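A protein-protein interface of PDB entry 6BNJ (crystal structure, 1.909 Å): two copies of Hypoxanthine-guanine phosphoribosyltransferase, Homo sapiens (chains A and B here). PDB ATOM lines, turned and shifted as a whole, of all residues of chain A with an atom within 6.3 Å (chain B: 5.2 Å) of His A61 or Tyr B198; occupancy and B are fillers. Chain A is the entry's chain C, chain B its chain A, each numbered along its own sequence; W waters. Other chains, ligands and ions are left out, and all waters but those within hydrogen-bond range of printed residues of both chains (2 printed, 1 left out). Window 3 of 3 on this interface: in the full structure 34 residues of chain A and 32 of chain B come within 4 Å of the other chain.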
ATOM      1  N   MET A  57      14.619 -23.798 -25.313  1.00  0.00           N
ATOM      2  CA  MET A  57      15.408 -22.560 -25.475  1.00  0.00           C
ATOM      3  C   MET A  57      15.963 -21.967 -24.201  1.00  0.00           C
ATOM      4  O   MET A  57      16.739 -21.018 -24.253  1.00  0.00           O
ATOM      5  CB  MET A  57      14.553 -21.478 -26.165  1.00  0.00           C
ATOM      6  CG  MET A  57      13.914 -21.974 -27.470  1.00  0.00           C
ATOM      7  SD  MET A  57      13.125 -20.714 -28.504  1.00  0.00           S
ATOM      8  CE  MET A  57      14.504 -19.738 -29.125  1.00  0.00           C
ATOM      9  N   GLY A  58      15.576 -22.500 -23.055  1.00  0.00           N
ATOM     10  CA  GLY A  58      15.876 -21.810 -21.816  1.00  0.00           C
ATOM     11  C   GLY A  58      17.307 -22.002 -21.375  1.00  0.00           C
ATOM     12  O   GLY A  58      17.637 -21.646 -20.255  1.00  0.00           O
ATOM     13  N   GLY A  59      18.157 -22.563 -22.237  1.00  0.00           N
ATOM     14  CA  GLY A  59      19.549 -22.770 -21.878  1.00  0.00           C
ATOM     15  C   GLY A  59      20.410 -21.513 -21.987  1.00  0.00           C
ATOM     16  O   GLY A  59      21.517 -21.446 -21.427  1.00  0.00           O
ATOM     17  N   HIS A  60      19.924 -20.517 -22.728  1.00  0.00           N
ATOM     18  CA  HIS A  60      20.758 -19.346 -23.035  1.00  0.00           C
ATOM     19  C   HIS A  60      19.876 -18.140 -23.211  1.00  0.00           C
ATOM     20  O   HIS A  60      18.741 -18.297 -23.618  1.00  0.00           O
ATOM     21  CB  HIS A  60      21.583 -19.592 -24.315  1.00  0.00           C
ATOM     22  CG  HIS A  60      22.550 -18.497 -24.636  1.00  0.00           C
ATOM     23  ND1 HIS A  60      23.777 -18.382 -24.015  1.00  0.00           N
ATOM     24  CD2 HIS A  60      22.481 -17.468 -25.514  1.00  0.00           C
ATOM     25  CE1 HIS A  60      24.414 -17.327 -24.483  1.00  0.00           C
ATOM     26  NE2 HIS A  60      23.648 -16.748 -25.393  1.00  0.00           N
ATOM     27  N   HIS A  61      20.388 -16.944 -22.916  1.00  0.00           N
ATOM     28  CA  HIS A  61      19.637 -15.721 -23.147  1.00  0.00           C
ATOM     29  C   HIS A  61      18.727 -15.787 -24.371  1.00  0.00           C
ATOM     30  O   HIS A  61      19.200 -16.025 -25.494  1.00  0.00           O
ATOM     31  CB  HIS A  61      20.624 -14.578 -23.302  1.00  0.00           C
ATOM     32  CG  HIS A  61      19.983 -13.244 -23.454  1.00  0.00           C
ATOM     33  ND1 HIS A  61      20.278 -12.192 -22.616  1.00  0.00           N
ATOM     34  CD2 HIS A  61      19.089 -12.773 -24.351  1.00  0.00           C
ATOM     35  CE1 HIS A  61      19.593 -11.128 -22.996  1.00  0.00           C
ATOM     36  NE2 HIS A  61      18.857 -11.454 -24.041  1.00  0.00           N
ATOM     37  N   ILE A  62      17.447 -15.513 -24.167  1.00  0.00           N
ATOM     38  CA  ILE A  62      16.477 -15.483 -25.256  1.00  0.00           C
ATOM     39  C   ILE A  62      16.160 -14.076 -25.731  1.00  0.00           C
ATOM     40  O   ILE A  62      15.938 -13.162 -24.910  1.00  0.00           O
ATOM     41  CB  ILE A  62      15.129 -16.174 -24.836  1.00  0.00           C
ATOM     42  CG1 ILE A  62      15.365 -17.677 -24.631  1.00  0.00           C
ATOM     43  CG2 ILE A  62      13.947 -15.871 -25.854  1.00  0.00           C
ATOM     44  CD1 ILE A  62      14.234 -18.363 -23.842  1.00  0.00           C
ATOM     45  N   VAL A  63      16.123 -13.897 -27.052  1.00  0.00           N
ATOM     46  CA  VAL A  63      15.583 -12.658 -27.621  1.00  0.00           C
ATOM     47  C   VAL A  63      14.268 -13.027 -28.282  1.00  0.00           C
ATOM     48  O   VAL A  63      14.222 -13.776 -29.258  1.00  0.00           O
ATOM     49  CB  VAL A  63      16.550 -11.951 -28.627  1.00  0.00           C
ATOM     50  CG1 VAL A  63      15.873 -10.715 -29.252  1.00  0.00           C
ATOM     51  CG2 VAL A  63      17.879 -11.524 -27.932  1.00  0.00           C
ATOM     52  N   ILE A  93      16.369 -17.965 -17.311  1.00  0.00           N
ATOM     53  CA  ILE A  93      17.296 -17.279 -18.175  1.00  0.00           C
ATOM     54  C   ILE A  93      16.718 -15.901 -18.496  1.00  0.00           C
ATOM     55  O   ILE A  93      15.487 -15.741 -18.540  1.00  0.00           O
ATOM     56  CB  ILE A  93      17.524 -18.134 -19.475  1.00  0.00           C
ATOM     57  CG1 ILE A  93      18.912 -17.904 -20.068  1.00  0.00           C
ATOM     58  CG2 ILE A  93      16.341 -17.992 -20.486  1.00  0.00           C
ATOM     59  CD1 ILE A  93      19.978 -18.675 -19.379  1.00  0.00           C
ATOM     60  N   PRO A  94      17.586 -14.888 -18.679  1.00  0.00           N
ATOM     61  CA  PRO A  94      17.078 -13.575 -19.080  1.00  0.00           C
ATOM     62  C   PRO A  94      16.447 -13.642 -20.450  1.00  0.00           C
ATOM     63  O   PRO A  94      16.862 -14.412 -21.328  1.00  0.00           O
ATOM     64  CB  PRO A  94      18.332 -12.698 -19.116  1.00  0.00           C
ATOM     65  CG  PRO A  94      19.346 -13.462 -18.392  1.00  0.00           C
ATOM     66  CD  PRO A  94      19.049 -14.884 -18.536  1.00  0.00           C
ATOM     67  N   MET A  95      15.409 -12.855 -20.625  1.00  0.00           N
ATOM     68  CA  MET A  95      14.856 -12.676 -21.944  1.00  0.00           C
ATOM     69  C   MET A  95      14.766 -11.174 -22.259  1.00  0.00           C
ATOM     70  O   MET A  95      14.347 -10.363 -21.402  1.00  0.00           O
ATOM     71  CB  MET A  95      13.498 -13.340 -22.045  1.00  0.00           C
ATOM     72  CG  MET A  95      12.797 -13.077 -23.335  1.00  0.00           C
ATOM     73  SD  MET A  95      11.104 -13.697 -23.293  1.00  0.00           S
ATOM     74  CE  MET A  95      11.292 -15.403 -22.813  1.00  0.00           C
ATOM     75  N   THR A  96      15.184 -10.785 -23.470  1.00  0.00           N
ATOM     76  CA  THR A  96      14.954  -9.400 -23.919  1.00  0.00           C
ATOM     77  C   THR A  96      13.938  -9.474 -25.072  1.00  0.00           C
ATOM     78  O   THR A  96      13.692 -10.551 -25.615  1.00  0.00           O
ATOM     79  CB  THR A  96      16.256  -8.723 -24.352  1.00  0.00           C
ATOM     80  OG1 THR A  96      16.958  -9.622 -25.196  1.00  0.00           O
ATOM     81  CG2 THR A  96      17.151  -8.468 -23.139  1.00  0.00           C
ATOM     82  N   GLY A 127      24.479 -14.470 -31.449  1.00  0.00           N
ATOM     83  CA  GLY A 127      24.824 -15.288 -30.286  1.00  0.00           C
ATOM     84  C   GLY A 127      23.683 -15.539 -29.292  1.00  0.00           C
ATOM     85  O   GLY A 127      23.914 -16.035 -28.175  1.00  0.00           O
ATOM     86  N   LYS A 128      22.456 -15.196 -29.667  1.00  0.00           N
ATOM     87  CA  LYS A 128      21.327 -15.316 -28.733  1.00  0.00           C
ATOM     88  C   LYS A 128      20.420 -16.432 -29.186  1.00  0.00           C
ATOM     89  O   LYS A 128      20.506 -16.863 -30.331  1.00  0.00           O
ATOM     90  CB  LYS A 128      20.537 -14.006 -28.638  1.00  0.00           C
ATOM     91  CG  LYS A 128      21.363 -12.834 -28.090  1.00  0.00           C
ATOM     92  CD  LYS A 128      21.790 -13.105 -26.640  1.00  0.00           C
ATOM     93  CE  LYS A 128      22.232 -11.825 -25.915  1.00  0.00           C
ATOM     94  NZ  LYS A 128      23.235 -11.020 -26.705  1.00  0.00           N
ATOM     95  N   ASN A 129      19.575 -16.914 -28.269  1.00  0.00           N
ATOM     96  CA  ASN A 129      18.486 -17.812 -28.626  1.00  0.00           C
ATOM     97  C   ASN A 129      17.294 -16.970 -29.090  1.00  0.00           C
ATOM     98  O   ASN A 129      16.608 -16.329 -28.290  1.00  0.00           O
ATOM     99  CB  ASN A 129      18.119 -18.714 -27.437  1.00  0.00           C
ATOM    100  CG  ASN A 129      19.136 -19.857 -27.223  1.00  0.00           C
ATOM    101  OD1 ASN A 129      20.135 -19.967 -27.952  1.00  0.00           O
ATOM    102  ND2 ASN A 129      18.879 -20.710 -26.232  1.00  0.00           N
ATOM    103  N   VAL A 130      17.024 -16.987 -30.389  1.00  0.00           N
ATOM    104  CA  VAL A 130      16.046 -16.048 -30.926  1.00  0.00           C
ATOM    105  C   VAL A 130      14.718 -16.747 -31.138  1.00  0.00           C
ATOM    106  O   VAL A 130      14.643 -17.782 -31.820  1.00  0.00           O
ATOM    107  CB  VAL A 130      16.554 -15.419 -32.263  1.00  0.00           C
ATOM    108  CG1 VAL A 130      15.480 -14.540 -32.922  1.00  0.00           C
ATOM    109  CG2 VAL A 130      17.819 -14.595 -31.988  1.00  0.00           C
ATOM    110  N   TYR B  28      17.294 -12.827 -11.683  1.00  0.00           N
ATOM    111  CA  TYR B  28      17.417 -11.451 -11.234  1.00  0.00           C
ATOM    112  C   TYR B  28      17.495 -11.366  -9.712  1.00  0.00           C
ATOM    113  O   TYR B  28      17.428 -10.272  -9.151  1.00  0.00           O
ATOM    114  CB  TYR B  28      16.223 -10.608 -11.719  1.00  0.00           C
ATOM    115  CG  TYR B  28      16.184 -10.281 -13.217  1.00  0.00           C
ATOM    116  CD1 TYR B  28      17.337  -9.943 -13.911  1.00  0.00           C
ATOM    117  CD2 TYR B  28      14.959 -10.238 -13.897  1.00  0.00           C
ATOM    118  CE1 TYR B  28      17.287  -9.617 -15.264  1.00  0.00           C
ATOM    119  CE2 TYR B  28      14.884  -9.895 -15.232  1.00  0.00           C
ATOM    120  CZ  TYR B  28      16.058  -9.599 -15.922  1.00  0.00           C
ATOM    121  OH  TYR B  28      15.978  -9.267 -17.240  1.00  0.00           O
ATOM    122  N   LEU B 193       9.609  -1.804 -18.260  1.00  0.00           N
ATOM    123  CA  LEU B 193      10.622  -0.745 -18.047  1.00  0.00           C
ATOM    124  C   LEU B 193      12.001  -1.386 -17.924  1.00  0.00           C
ATOM    125  O   LEU B 193      12.215  -2.268 -17.078  1.00  0.00           O
ATOM    126  CB  LEU B 193      10.299   0.093 -16.799  1.00  0.00           C
ATOM    127  CG  LEU B 193       9.132   1.038 -17.140  1.00  0.00           C
ATOM    128  CD1 LEU B 193       7.832   0.483 -16.673  1.00  0.00           C
ATOM    129  CD2 LEU B 193       9.346   2.432 -16.561  1.00  0.00           C
ATOM    130  N   ASP B 194      12.929  -0.959 -18.758  1.00  0.00           N
ATOM    131  CA  ASP B 194      14.203  -1.641 -18.802  1.00  0.00           C
ATOM    132  C   ASP B 194      15.360  -0.843 -18.227  1.00  0.00           C
ATOM    133  O   ASP B 194      15.318   0.381 -18.110  1.00  0.00           O
ATOM    134  CB  ASP B 194      14.544  -1.984 -20.253  1.00  0.00           C
ATOM    135  CG  ASP B 194      14.974  -0.757 -21.052  1.00  0.00           C
ATOM    136  OD1 ASP B 194      14.186   0.205 -21.139  1.00  0.00           O
ATOM    137  OD2 ASP B 194      16.096  -0.753 -21.587  1.00  0.00           O
ATOM    138  N   TYR B 195      16.443  -1.560 -17.995  1.00  0.00           N
ATOM    139  CA  TYR B 195      17.764  -1.010 -17.815  1.00  0.00           C
ATOM    140  C   TYR B 195      18.674  -1.689 -18.844  1.00  0.00           C
ATOM    141  O   TYR B 195      18.949  -2.878 -18.736  1.00  0.00           O
ATOM    142  CB  TYR B 195      18.241  -1.251 -16.382  1.00  0.00           C
ATOM    143  CG  TYR B 195      19.643  -0.814 -16.064  1.00  0.00           C
ATOM    144  CD1 TYR B 195      19.997   0.530 -16.028  1.00  0.00           C
ATOM    145  CD2 TYR B 195      20.638  -1.767 -15.797  1.00  0.00           C
ATOM    146  CE1 TYR B 195      21.318   0.929 -15.716  1.00  0.00           C
ATOM    147  CE2 TYR B 195      21.928  -1.382 -15.462  1.00  0.00           C
ATOM    148  CZ  TYR B 195      22.262  -0.023 -15.427  1.00  0.00           C
ATOM    149  OH  TYR B 195      23.548   0.344 -15.110  1.00  0.00           O
ATOM    150  N   ASN B 196      19.119  -0.924 -19.832  1.00  0.00           N
ATOM    151  CA  ASN B 196      19.843  -1.479 -20.968  1.00  0.00           C
ATOM    152  C   ASN B 196      19.233  -2.770 -21.510  1.00  0.00           C
ATOM    153  O   ASN B 196      19.947  -3.748 -21.772  1.00  0.00           O
ATOM    154  CB  ASN B 196      21.295  -1.678 -20.585  1.00  0.00           C
ATOM    155  CG  ASN B 196      21.943  -0.394 -20.234  1.00  0.00           C
ATOM    156  OD1 ASN B 196      21.864   0.572 -20.996  1.00  0.00           O
ATOM    157  ND2 ASN B 196      22.553  -0.335 -19.058  1.00  0.00           N
ATOM    158  N   GLU B 197      17.899  -2.738 -21.644  1.00  0.00           N
ATOM    159  CA  GLU B 197      17.057  -3.791 -22.263  1.00  0.00           C
ATOM    160  C   GLU B 197      16.734  -4.960 -21.313  1.00  0.00           C
ATOM    161  O   GLU B 197      15.881  -5.781 -21.626  1.00  0.00           O
ATOM    162  CB  GLU B 197      17.702  -4.346 -23.547  1.00  0.00           C
ATOM    163  CG  GLU B 197      17.794  -3.338 -24.697  1.00  0.00           C
ATOM    164  CD  GLU B 197      16.437  -2.746 -25.092  1.00  0.00           C
ATOM    165  OE1 GLU B 197      15.408  -3.437 -25.020  1.00  0.00           O
ATOM    166  OE2 GLU B 197      16.393  -1.570 -25.492  1.00  0.00           O
ATOM    167  N   TYR B 198      17.419  -5.026 -20.175  1.00  0.00           N
ATOM    168  CA  TYR B 198      17.074  -6.003 -19.140  1.00  0.00           C
ATOM    169  C   TYR B 198      15.886  -5.570 -18.285  1.00  0.00           C
ATOM    170  O   TYR B 198      15.543  -4.386 -18.275  1.00  0.00           O
ATOM    171  CB  TYR B 198      18.278  -6.253 -18.252  1.00  0.00           C
ATOM    172  CG  TYR B 198      19.350  -7.017 -18.982  1.00  0.00           C
ATOM    173  CD1 TYR B 198      19.346  -8.415 -18.992  1.00  0.00           C
ATOM    174  CD2 TYR B 198      20.347  -6.357 -19.676  1.00  0.00           C
ATOM    175  CE1 TYR B 198      20.314  -9.121 -19.666  1.00  0.00           C
ATOM    176  CE2 TYR B 198      21.333  -7.056 -20.351  1.00  0.00           C
ATOM    177  CZ  TYR B 198      21.313  -8.436 -20.342  1.00  0.00           C
ATOM    178  OH  TYR B 198      22.285  -9.136 -21.010  1.00  0.00           O
ATOM    179  N   PHE B 199      15.301  -6.543 -17.575  1.00  0.00           N
ATOM    180  CA  PHE B 199      14.216  -6.348 -16.609  1.00  0.00           C
ATOM    181  C   PHE B 199      12.878  -6.089 -17.283  1.00  0.00           C
ATOM    182  O   PHE B 199      11.919  -5.830 -16.584  1.00  0.00           O
ATOM    183  CB  PHE B 199      14.513  -5.192 -15.624  1.00  0.00           C
ATOM    184  CG  PHE B 199      15.797  -5.360 -14.822  1.00  0.00           C
ATOM    185  CD1 PHE B 199      15.948  -6.408 -13.909  1.00  0.00           C
ATOM    186  CD2 PHE B 199      16.831  -4.446 -14.960  1.00  0.00           C
ATOM    187  CE1 PHE B 199      17.118  -6.548 -13.166  1.00  0.00           C
ATOM    188  CE2 PHE B 199      17.999  -4.574 -14.213  1.00  0.00           C
ATOM    189  CZ  PHE B 199      18.135  -5.629 -13.304  1.00  0.00           C
ATOM    190  N   ARG B 200      12.778  -6.186 -18.620  1.00  0.00           N
ATOM    191  CA  ARG B 200      11.461  -6.137 -19.212  1.00  0.00           C
ATOM    192  C   ARG B 200      10.691  -7.418 -18.906  1.00  0.00           C
ATOM    193  O   ARG B 200       9.455  -7.391 -18.847  1.00  0.00           O
ATOM    194  CB  ARG B 200      11.516  -5.905 -20.744  1.00  0.00           C
ATOM    195  CG  ARG B 200      12.212  -4.614 -21.123  1.00  0.00           C
ATOM    196  CD  ARG B 200      11.790  -4.176 -22.548  1.00  0.00           C
ATOM    197  NE  ARG B 200      12.752  -3.280 -23.168  1.00  0.00           N
ATOM    198  CZ  ARG B 200      12.676  -1.963 -23.153  1.00  0.00           C
ATOM    199  NH1 ARG B 200      11.657  -1.369 -22.515  1.00  0.00           N
ATOM    200  NH2 ARG B 200      13.617  -1.242 -23.783  1.00  0.00           N
ATOM    201  N   ASP B 201      11.397  -8.516 -18.711  1.00  0.00           N
ATOM    202  CA  ASP B 201      10.807  -9.824 -18.404  1.00  0.00           C
ATOM    203  C   ASP B 201      10.574 -10.024 -16.879  1.00  0.00           C
ATOM    204  O   ASP B 201      11.031 -10.998 -16.301  1.00  0.00           O
ATOM    205  CB  ASP B 201      11.707 -10.955 -18.922  1.00  0.00           C
ATOM    206  CG  ASP B 201      13.140 -10.849 -18.394  1.00  0.00           C
ATOM    207  OD1 ASP B 201      13.581  -9.728 -18.114  1.00  0.00           O
ATOM    208  OD2 ASP B 201      13.861 -11.867 -18.286  1.00  0.00           O
ATOM    209  N   TYR B 216      24.506  -5.246 -15.585  1.00  0.00           N
ATOM    210  CA  TYR B 216      23.840  -5.024 -16.877  1.00  0.00           C
ATOM    211  C   TYR B 216      24.218  -3.672 -17.424  1.00  0.00           C
ATOM    212  O   TYR B 216      23.571  -3.176 -18.337  1.00  0.00           O
ATOM    213  CB  TYR B 216      22.305  -5.151 -16.753  1.00  0.00           C
ATOM    214  CG  TYR B 216      21.894  -6.505 -16.209  1.00  0.00           C
ATOM    215  CD1 TYR B 216      22.216  -7.666 -16.884  1.00  0.00           C
ATOM    216  CD2 TYR B 216      21.208  -6.617 -15.003  1.00  0.00           C
ATOM    217  CE1 TYR B 216      21.874  -8.922 -16.379  1.00  0.00           C
ATOM    218  CE2 TYR B 216      20.844  -7.864 -14.492  1.00  0.00           C
ATOM    219  CZ  TYR B 216      21.184  -9.016 -15.189  1.00  0.00           C
ATOM    220  OH  TYR B 216      20.849 -10.271 -14.692  1.00  0.00           O
HETATM  221  O   HOH W   1      22.285 -11.906 -20.742  1.00  0.00           O
HETATM  222  O   HOH W   2      13.043 -14.299 -18.976  1.00  0.00           O
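The backbone NH of Met A95 sits at hydrogen-bond distance from the side-chain carboxylate of Asp B201.
N of Thr A96 lies within hydrogen-bond range of O of Ile A62 (2.9 Å). A ring nitrogen (NE2) of His A61 lies within hydrogen-bond range of the side-chain hydroxyl (OG1) of Thr A96 (2.9 Å). OD1 of Asp B201 sits at hydrogen-bond distance from OH of Tyr B28 (2.6 Å). The backbone NH (N) of Ile A62 sits at hydrogen-bond distance from the backbone carbonyl oxygen (O) of Pro A94, 3.1 Å away. NH2 of Arg B200 lies within salt-bridge range of OE1 of Glu B197, 3.1 Å away. The backbone carbonyl oxygen (O) of His A61 lies within hydrogen-bond range of the backbone NH (N) of Asn A129, 2.9 Å away.
His A61 touches Tyr B198. Asp B201 touches Pro A94. Thr A96 touches Glu B197.
His A61 touches just one residue of chain B: Tyr B198. Printed residues of chain A within 4 Å of Asp B201: Pro A94 (3.7 Å) and Met A95 (3.0 Å). Of the printed residues of chain B, Met A95 touches Asp B201. Of the printed residues of chain B, Thr A96 touches Glu B197. Tyr B195 touches none of the printed residues of chain A. The nearest printed residue of chain B that does not touch Pro A94 is Tyr B198 (4.1 Å).
Of the 15 printed residues of chain A, 4 touch a printed residue of chain B. Along chain A the printed residues that touch a printed residue of chain B span positions 61 to 96. Hydrophobic or aromatic side chains of chain B that line the printed part of chain A: Tyr B198. Along chain B the printed residues that touch a printed residue of chain A span positions 197 to 201. Among the printed residues, 4 pairs touch across the chains. Among the printed residues, no Asp or Glu carboxylate lies within 4 Å of a Lys or Arg side-chain nitrogen of the other chain.
No position is printed for both chains.
Water W2 lies within hydrogen-bond range of OD2 of Asp B201 (2.7 Å), O of Ile A93 (2.9 Å) and N of Met A95 (3.2 Å). Water W1 lies within hydrogen-bond range of ND1 of His A61 (2.8 Å) and OH of Tyr B198 (2.8 Å).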
